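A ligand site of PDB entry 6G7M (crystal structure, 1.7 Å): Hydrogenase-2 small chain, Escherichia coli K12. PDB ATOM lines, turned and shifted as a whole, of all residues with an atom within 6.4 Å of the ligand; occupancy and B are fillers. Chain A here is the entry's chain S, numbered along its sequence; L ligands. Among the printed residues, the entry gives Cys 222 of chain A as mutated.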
ATOM      1  N   ILE A 191     -21.776  27.839  16.054  1.00  0.00           N
ATOM      2  CA  ILE A 191     -22.175  26.687  16.898  1.00  0.00           C
ATOM      3  C   ILE A 191     -21.597  25.383  16.349  1.00  0.00           C
ATOM      4  O   ILE A 191     -21.088  24.558  17.120  1.00  0.00           O
ATOM      5  CB  ILE A 191     -23.725  26.654  17.053  1.00  0.00           C
ATOM      6  CG1 ILE A 191     -24.170  27.861  17.900  1.00  0.00           C
ATOM      7  CG2 ILE A 191     -24.190  25.351  17.700  1.00  0.00           C
ATOM      8  CD1 ILE A 191     -25.681  28.087  17.899  1.00  0.00           C
ATOM      9  N   HIS A 192     -21.678  25.175  15.023  1.00  0.00           N
ATOM     10  CA  HIS A 192     -21.164  23.952  14.373  1.00  0.00           C
ATOM     11  C   HIS A 192     -19.642  23.788  14.483  1.00  0.00           C
ATOM     12  O   HIS A 192     -19.149  22.649  14.377  1.00  0.00           O
ATOM     13  CB  HIS A 192     -21.627  23.961  12.919  1.00  0.00           C
ATOM     14  CG  HIS A 192     -21.205  22.797  12.077  1.00  0.00           C
ATOM     15  ND1 HIS A 192     -21.786  21.542  12.172  1.00  0.00           N
ATOM     16  CD2 HIS A 192     -20.296  22.724  11.064  1.00  0.00           C
ATOM     17  CE1 HIS A 192     -21.261  20.761  11.246  1.00  0.00           C
ATOM     18  NE2 HIS A 192     -20.350  21.439  10.570  1.00  0.00           N
ATOM     19  N   GLU A 193     -18.940  24.888  14.726  1.00  0.00           N
ATOM     20  CA  GLU A 193     -17.488  24.862  14.925  1.00  0.00           C
ATOM     21  C   GLU A 193     -17.141  24.650  16.390  1.00  0.00           C
ATOM     22  O   GLU A 193     -15.948  24.738  16.771  1.00  0.00           O
ATOM     23  CB  GLU A 193     -16.785  26.091  14.317  1.00  0.00           C
ATOM     24  CG  GLU A 193     -16.903  26.140  12.789  1.00  0.00           C
ATOM     25  CD  GLU A 193     -16.317  24.914  12.099  1.00  0.00           C
ATOM     26  OE1 GLU A 193     -17.019  24.215  11.338  1.00  0.00           O
ATOM     27  OE2 GLU A 193     -15.140  24.591  12.340  1.00  0.00           O
ATOM     28  N   CYS A 195     -19.520  22.118  18.314  1.00  0.00           N
ATOM     29  CA  CYS A 195     -20.660  21.285  18.645  1.00  0.00           C
ATOM     30  C   CYS A 195     -20.220  19.856  18.954  1.00  0.00           C
ATOM     31  O   CYS A 195     -19.431  19.252  18.177  1.00  0.00           O
ATOM     32  CB  CYS A 195     -21.683  21.241  17.487  1.00  0.00           C
ATOM     33  SG  CYS A 195     -23.148  20.150  17.857  1.00  0.00           S
ATOM     34  N   GLU A 196     -20.697  19.306  20.082  1.00  0.00           N
ATOM     35  CA  GLU A 196     -20.314  17.952  20.519  1.00  0.00           C
ATOM     36  C   GLU A 196     -20.820  16.844  19.581  1.00  0.00           C
ATOM     37  O   GLU A 196     -20.379  15.680  19.710  1.00  0.00           O
ATOM     38  CB  GLU A 196     -20.741  17.722  21.987  1.00  0.00           C
ATOM     39  CG  GLU A 196     -22.246  17.595  22.261  1.00  0.00           C
ATOM     40  CD  GLU A 196     -23.003  18.905  22.513  1.00  0.00           C
ATOM     41  OE1 GLU A 196     -22.481  20.005  22.171  1.00  0.00           O
ATOM     42  OE2 GLU A 196     -24.188  18.808  22.995  1.00  0.00           O
ATOM     43  N   ARG A 197     -21.747  17.180  18.660  1.00  0.00           N
ATOM     44  CA  ARG A 197     -22.222  16.190  17.688  1.00  0.00           C
ATOM     45  C   ARG A 197     -21.435  16.193  16.373  1.00  0.00           C
ATOM     46  O   ARG A 197     -21.758  15.437  15.449  1.00  0.00           O
ATOM     47  CB  ARG A 197     -23.703  16.319  17.437  1.00  0.00           C
ATOM     48  CG  ARG A 197     -24.485  16.159  18.763  1.00  0.00           C
ATOM     49  CD  ARG A 197     -25.963  15.913  18.587  1.00  0.00           C
ATOM     50  NE  ARG A 197     -26.588  15.695  19.890  1.00  0.00           N
ATOM     51  CZ  ARG A 197     -27.766  15.140  20.111  1.00  0.00           C
ATOM     52  NH1 ARG A 197     -28.542  14.769  19.089  1.00  0.00           N
ATOM     53  NH2 ARG A 197     -28.184  14.993  21.362  1.00  0.00           N
ATOM     54  N   ARG A 198     -20.397  17.013  16.312  1.00  0.00           N
ATOM     55  CA  ARG A 198     -19.563  17.073  15.109  1.00  0.00           C
ATOM     56  C   ARG A 198     -18.985  15.737  14.674  1.00  0.00           C
ATOM     57  O   ARG A 198     -18.885  15.495  13.457  1.00  0.00           O
ATOM     58  CB  ARG A 198     -18.451  18.131  15.207  1.00  0.00           C
ATOM     59  CG  ARG A 198     -17.545  18.239  13.965  1.00  0.00           C
ATOM     60  CD  ARG A 198     -18.336  18.681  12.715  1.00  0.00           C
ATOM     61  NE  ARG A 198     -17.375  18.976  11.669  1.00  0.00           N
ATOM     62  CZ  ARG A 198     -16.805  20.171  11.442  1.00  0.00           C
ATOM     63  NH1 ARG A 198     -17.187  21.276  12.106  1.00  0.00           N
ATOM     64  NH2 ARG A 198     -15.840  20.250  10.536  1.00  0.00           N
ATOM     65  N   PRO A 199     -18.566  14.867  15.638  1.00  0.00           N
ATOM     66  CA  PRO A 199     -18.073  13.548  15.182  1.00  0.00           C
ATOM     67  C   PRO A 199     -19.092  12.717  14.373  1.00  0.00           C
ATOM     68  O   PRO A 199     -18.728  12.011  13.422  1.00  0.00           O
ATOM     69  CB  PRO A 199     -17.716  12.844  16.490  1.00  0.00           C
ATOM     70  CG  PRO A 199     -17.443  13.964  17.498  1.00  0.00           C
ATOM     71  CD  PRO A 199     -18.414  15.051  17.089  1.00  0.00           C
ATOM     72  N   PHE A 201     -21.675  14.033  12.547  1.00  0.00           N
ATOM     73  CA  PHE A 201     -21.677  14.738  11.250  1.00  0.00           C
ATOM     74  C   PHE A 201     -20.532  14.193  10.377  1.00  0.00           C
ATOM     75  O   PHE A 201     -20.740  13.794   9.217  1.00  0.00           O
ATOM     76  CB  PHE A 201     -21.455  16.226  11.482  1.00  0.00           C
ATOM     77  CG  PHE A 201     -21.402  17.065  10.209  1.00  0.00           C
ATOM     78  CD1 PHE A 201     -20.198  17.321   9.584  1.00  0.00           C
ATOM     79  CD2 PHE A 201     -22.559  17.668   9.716  1.00  0.00           C
ATOM     80  CE1 PHE A 201     -20.143  18.100   8.431  1.00  0.00           C
ATOM     81  CE2 PHE A 201     -22.511  18.464   8.579  1.00  0.00           C
ATOM     82  CZ  PHE A 201     -21.299  18.689   7.941  1.00  0.00           C
ATOM     83  N   PHE A 206     -26.474  10.445  10.988  1.00  0.00           N
ATOM     84  CA  PHE A 206     -27.515  11.495  11.025  1.00  0.00           C
ATOM     85  C   PHE A 206     -28.866  10.934  11.446  1.00  0.00           C
ATOM     86  O   PHE A 206     -29.298   9.880  10.952  1.00  0.00           O
ATOM     87  CB  PHE A 206     -27.696  12.168   9.642  1.00  0.00           C
ATOM     88  CG  PHE A 206     -26.463  12.866   9.101  1.00  0.00           C
ATOM     89  CD1 PHE A 206     -26.003  14.059   9.653  1.00  0.00           C
ATOM     90  CD2 PHE A 206     -25.832  12.384   7.948  1.00  0.00           C
ATOM     91  CE1 PHE A 206     -24.910  14.739   9.112  1.00  0.00           C
ATOM     92  CE2 PHE A 206     -24.732  13.058   7.410  1.00  0.00           C
ATOM     93  CZ  PHE A 206     -24.262  14.229   7.991  1.00  0.00           C
ATOM     94  N   TRP A 219     -27.265  11.273  17.681  1.00  0.00           N
ATOM     95  CA  TRP A 219     -26.549  11.606  16.439  1.00  0.00           C
ATOM     96  C   TRP A 219     -26.795  13.034  15.959  1.00  0.00           C
ATOM     97  O   TRP A 219     -27.633  13.779  16.509  1.00  0.00           O
ATOM     98  CB  TRP A 219     -26.923  10.571  15.327  1.00  0.00           C
ATOM     99  CG  TRP A 219     -26.351   9.188  15.500  1.00  0.00           C
ATOM    100  CD1 TRP A 219     -25.646   8.711  16.558  1.00  0.00           C
ATOM    101  CD2 TRP A 219     -26.489   8.098  14.574  1.00  0.00           C
ATOM    102  NE1 TRP A 219     -25.339   7.368  16.355  1.00  0.00           N
ATOM    103  CE2 TRP A 219     -25.841   6.985  15.148  1.00  0.00           C
ATOM    104  CE3 TRP A 219     -27.098   7.966  13.325  1.00  0.00           C
ATOM    105  CZ2 TRP A 219     -25.775   5.718  14.497  1.00  0.00           C
ATOM    106  CZ3 TRP A 219     -27.017   6.713  12.666  1.00  0.00           C
ATOM    107  CH2 TRP A 219     -26.355   5.614  13.263  1.00  0.00           C
ATOM    108  N   CYS A 220     -26.050  13.457  14.945  1.00  0.00           N
ATOM    109  CA  CYS A 220     -26.129  14.819  14.436  1.00  0.00           C
ATOM    110  C   CYS A 220     -27.504  15.116  13.856  1.00  0.00           C
ATOM    111  O   CYS A 220     -28.121  14.227  13.224  1.00  0.00           O
ATOM    112  CB  CYS A 220     -25.040  15.053  13.392  1.00  0.00           C
ATOM    113  SG  CYS A 220     -25.123  16.553  12.362  1.00  0.00           S
ATOM    114  N   LEU A 221     -27.955  16.368  14.060  1.00  0.00           N
ATOM    115  CA  LEU A 221     -29.283  16.810  13.595  1.00  0.00           C
ATOM    116  C   LEU A 221     -29.292  17.598  12.280  1.00  0.00           C
ATOM    117  O   LEU A 221     -30.313  18.251  11.929  1.00  0.00           O
ATOM    118  CB  LEU A 221     -29.986  17.579  14.722  1.00  0.00           C
ATOM    119  CG  LEU A 221     -29.958  16.886  16.100  1.00  0.00           C
ATOM    120  CD1 LEU A 221     -30.728  17.737  17.135  1.00  0.00           C
ATOM    121  CD2 LEU A 221     -30.537  15.475  16.045  1.00  0.00           C
ATOM    122  N   CYS A 222     -28.180  17.591  11.547  1.00  0.00           N
ATOM    123  CA  CYS A 222     -28.076  18.375  10.302  1.00  0.00           C
ATOM    124  C   CYS A 222     -29.228  18.091   9.320  1.00  0.00           C
ATOM    125  O   CYS A 222     -29.804  19.045   8.759  1.00  0.00           O
ATOM    126  CB  CYS A 222     -26.765  18.023   9.553  1.00  0.00           C
ATOM    127  SG  CYS A 222     -26.398  19.107   8.155  1.00  0.00           S
ATOM    128  N   HIS A 223     -29.555  16.810   9.109  1.00  0.00           N
ATOM    129  CA  HIS A 223     -30.617  16.454   8.160  1.00  0.00           C
ATOM    130  C   HIS A 223     -32.029  16.724   8.645  1.00  0.00           C
ATOM    131  O   HIS A 223     -32.954  16.645   7.848  1.00  0.00           O
ATOM    132  CB  HIS A 223     -30.417  15.040   7.582  1.00  0.00           C
ATOM    133  CG  HIS A 223     -29.196  14.931   6.713  1.00  0.00           C
ATOM    134  ND1 HIS A 223     -28.746  13.738   6.186  1.00  0.00           N
ATOM    135  CD2 HIS A 223     -28.297  15.867   6.315  1.00  0.00           C
ATOM    136  CE1 HIS A 223     -27.642  13.949   5.494  1.00  0.00           C
ATOM    137  NE2 HIS A 223     -27.345  15.237   5.555  1.00  0.00           N
ATOM    138  N   CYS A 226     -30.813  21.479  11.204  1.00  0.00           N
ATOM    139  CA  CYS A 226     -29.926  22.241  12.111  1.00  0.00           C
ATOM    140  C   CYS A 226     -29.228  23.403  11.430  1.00  0.00           C
ATOM    141  O   CYS A 226     -28.551  23.233  10.391  1.00  0.00           O
ATOM    142  CB  CYS A 226     -28.920  21.314  12.768  1.00  0.00           C
ATOM    143  SG  CYS A 226     -27.997  22.070  14.127  1.00  0.00           S
ATOM    144  N   LYS A 227     -29.341  24.595  12.026  1.00  0.00           N
ATOM    145  CA  LYS A 227     -28.737  25.819  11.526  1.00  0.00           C
ATOM    146  C   LYS A 227     -27.419  26.145  12.212  1.00  0.00           C
ATOM    147  O   LYS A 227     -26.813  27.211  11.980  1.00  0.00           O
ATOM    148  CB  LYS A 227     -29.715  26.994  11.613  1.00  0.00           C
ATOM    149  CG  LYS A 227     -31.063  26.740  10.967  1.00  0.00           C
ATOM    150  CD  LYS A 227     -30.935  26.367   9.475  1.00  0.00           C
ATOM    151  CE  LYS A 227     -32.281  26.318   8.768  1.00  0.00           C
ATOM    152  NZ  LYS A 227     -33.258  25.388   9.419  1.00  0.00           N
ATOM    153  N   GLY A 228     -26.947  25.216  13.056  1.00  0.00           N
ATOM    154  CA  GLY A 228     -25.592  25.366  13.660  1.00  0.00           C
ATOM    155  C   GLY A 228     -24.479  25.805  12.679  1.00  0.00           C
ATOM    156  O   GLY A 228     -23.637  26.624  13.046  1.00  0.00           O
ATOM    157  N   PRO A 229     -24.462  25.261  11.441  1.00  0.00           N
ATOM    158  CA  PRO A 229     -23.394  25.632  10.470  1.00  0.00           C
ATOM    159  C   PRO A 229     -23.353  27.101  10.034  1.00  0.00           C
ATOM    160  O   PRO A 229     -22.323  27.526   9.479  1.00  0.00           O
ATOM    161  CB  PRO A 229     -23.649  24.676   9.275  1.00  0.00           C
ATOM    162  CG  PRO A 229     -24.294  23.476   9.896  1.00  0.00           C
ATOM    163  CD  PRO A 229     -25.186  24.026  10.992  1.00  0.00           C
ATOM    164  N   TRP A 247     -29.338  22.385  26.077  1.00  0.00           N
ATOM    165  CA  TRP A 247     -29.520  23.297  24.926  1.00  0.00           C
ATOM    166  C   TRP A 247     -30.369  22.577  23.895  1.00  0.00           C
ATOM    167  O   TRP A 247     -30.607  21.392  24.081  1.00  0.00           O
ATOM    168  CB  TRP A 247     -28.186  23.817  24.358  1.00  0.00           C
ATOM    169  CG  TRP A 247     -27.249  22.878  23.653  1.00  0.00           C
ATOM    170  CD1 TRP A 247     -26.543  21.813  24.161  1.00  0.00           C
ATOM    171  CD2 TRP A 247     -26.876  22.956  22.239  1.00  0.00           C
ATOM    172  NE1 TRP A 247     -25.714  21.267  23.173  1.00  0.00           N
ATOM    173  CE2 TRP A 247     -25.916  21.931  21.989  1.00  0.00           C
ATOM    174  CE3 TRP A 247     -27.193  23.813  21.215  1.00  0.00           C
ATOM    175  CZ2 TRP A 247     -25.328  21.756  20.729  1.00  0.00           C
ATOM    176  CZ3 TRP A 247     -26.599  23.669  19.994  1.00  0.00           C
ATOM    177  CH2 TRP A 247     -25.670  22.630  19.757  1.00  0.00           C
ATOM    178  N   VAL A 249     -30.106  21.246  20.835  1.00  0.00           N
ATOM    179  CA  VAL A 249     -29.584  20.043  20.173  1.00  0.00           C
ATOM    180  C   VAL A 249     -29.418  18.921  21.209  1.00  0.00           C
ATOM    181  O   VAL A 249     -29.801  17.739  20.938  1.00  0.00           O
ATOM    182  CB  VAL A 249     -28.280  20.382  19.425  1.00  0.00           C
ATOM    183  CG1 VAL A 249     -27.515  19.124  19.048  1.00  0.00           C
ATOM    184  CG2 VAL A 249     -28.576  21.261  18.200  1.00  0.00           C
ATOM    185  N   PRO A 254     -33.075  20.378  16.339  1.00  0.00           N
ATOM    186  CA  PRO A 254     -32.046  21.181  15.655  1.00  0.00           C
ATOM    187  C   PRO A 254     -32.046  22.651  16.085  1.00  0.00           C
ATOM    188  O   PRO A 254     -33.097  23.188  16.530  1.00  0.00           O
ATOM    189  CB  PRO A 254     -32.459  21.065  14.147  1.00  0.00           C
ATOM    190  CG  PRO A 254     -33.913  20.710  14.193  1.00  0.00           C
ATOM    191  CD  PRO A 254     -34.027  19.785  15.366  1.00  0.00           C
ATOM    192  N   CYS A 255     -30.889  23.305  15.988  1.00  0.00           N
ATOM    193  CA  CYS A 255     -30.817  24.765  16.090  1.00  0.00           C
ATOM    194  C   CYS A 255     -31.657  25.340  14.936  1.00  0.00           C
ATOM    195  O   CYS A 255     -31.620  24.799  13.801  1.00  0.00           O
ATOM    196  CB  CYS A 255     -29.355  25.242  16.033  1.00  0.00           C
ATOM    197  SG  CYS A 255     -29.067  27.021  15.855  1.00  0.00           S
HETATM  198 FE1  LIG L   1     -24.740  18.461  13.605  1.00  0.00          FE
HETATM  199 FE2  LIG L   1     -26.014  20.864  14.188  1.00  0.00          FE
HETATM  200 FE3  LIG L   1     -23.412  20.811  13.265  1.00  0.00          FE
HETATM  201 FE4  LIG L   1     -24.007  19.973  15.783  1.00  0.00          FE
HETATM  202  S1  LIG L   1     -24.279  22.129  14.958  1.00  0.00           S
HETATM  203  S2  LIG L   1     -22.611  18.892  14.273  1.00  0.00           S
HETATM  204  S3  LIG L   1     -26.013  18.966  15.484  1.00  0.00           S
HETATM  205  S4  LIG L   1     -25.236  20.148  12.101  1.00  0.00           S
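ND1 of His 192 binds FE3 of the ligand (2.1 Å).
The side-chain sulfur of Cys 195 is bound to an iron atom (FE4) of the ligand (2.3 Å).
The side-chain sulfur of Cys 220 binds an iron atom (FE1) of the ligand (2.3 Å).
The side-chain sulfur (SG) of Cys 226 is bound to an iron atom (FE2) of the ligand, 2.3 Å away.
The backbone NH (N) of Leu 221 lies close to a sulfur (S3) of the ligand.
The backbone NH (N) of Arg 198 sits close to a sulfur (S2) of the ligand (3.5 Å).
The backbone carbonyl oxygen (O) of His 192 sits at hydrogen-bond distance from the guanidinium group (NH1) of Arg 198.
N of His 192 sits at hydrogen-bond distance from O of Gly 228, at 3.1 Å.
The side-chain sulfur of Cys 195 lies close to the backbone NH of Arg 197 (3.4 Å).
The backbone carbonyl oxygen (O) of Leu 221 is in hydrogen-bond range of the backbone NH (N) of Cys 226 (3.3 Å).
The side-chain sulfur (SG) of Cys 226 lies close to the backbone NH (N) of Gly 228 (3.5 Å).
The side-chain carboxylate (OE1) of Glu 193 lies within salt-bridge range of the guanidinium group (NH1) of Arg 198.
The backbone carbonyl oxygen of Val 249 lies within hydrogen-bond range of the guanidinium group of Arg 197.
NH1 of Arg 197 sits at hydrogen-bond distance from O of Trp 219, 2.9 Å away.
S2 of the ligand sits close to O of Arg 197.
CB of Cys 222 touches S4 of the ligand (3.7 Å).
Gly 228 touches the ligand (CA to S1, 3.7 Å).
Val 249 touches the ligand.
Hydrophobic or aromatic side chains within 4 Å of the ligand: His 192 and Val 249.
Ten residues have an atom within 4 Å of the ligand: His 192, Cys 195, Arg 197, Arg 198, Cys 220, Leu 221, Cys 222, Cys 226, Gly 228 and Val 249.
The nearest printed residue that does not touch the ligand is Phe 201 (4.03 Å).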
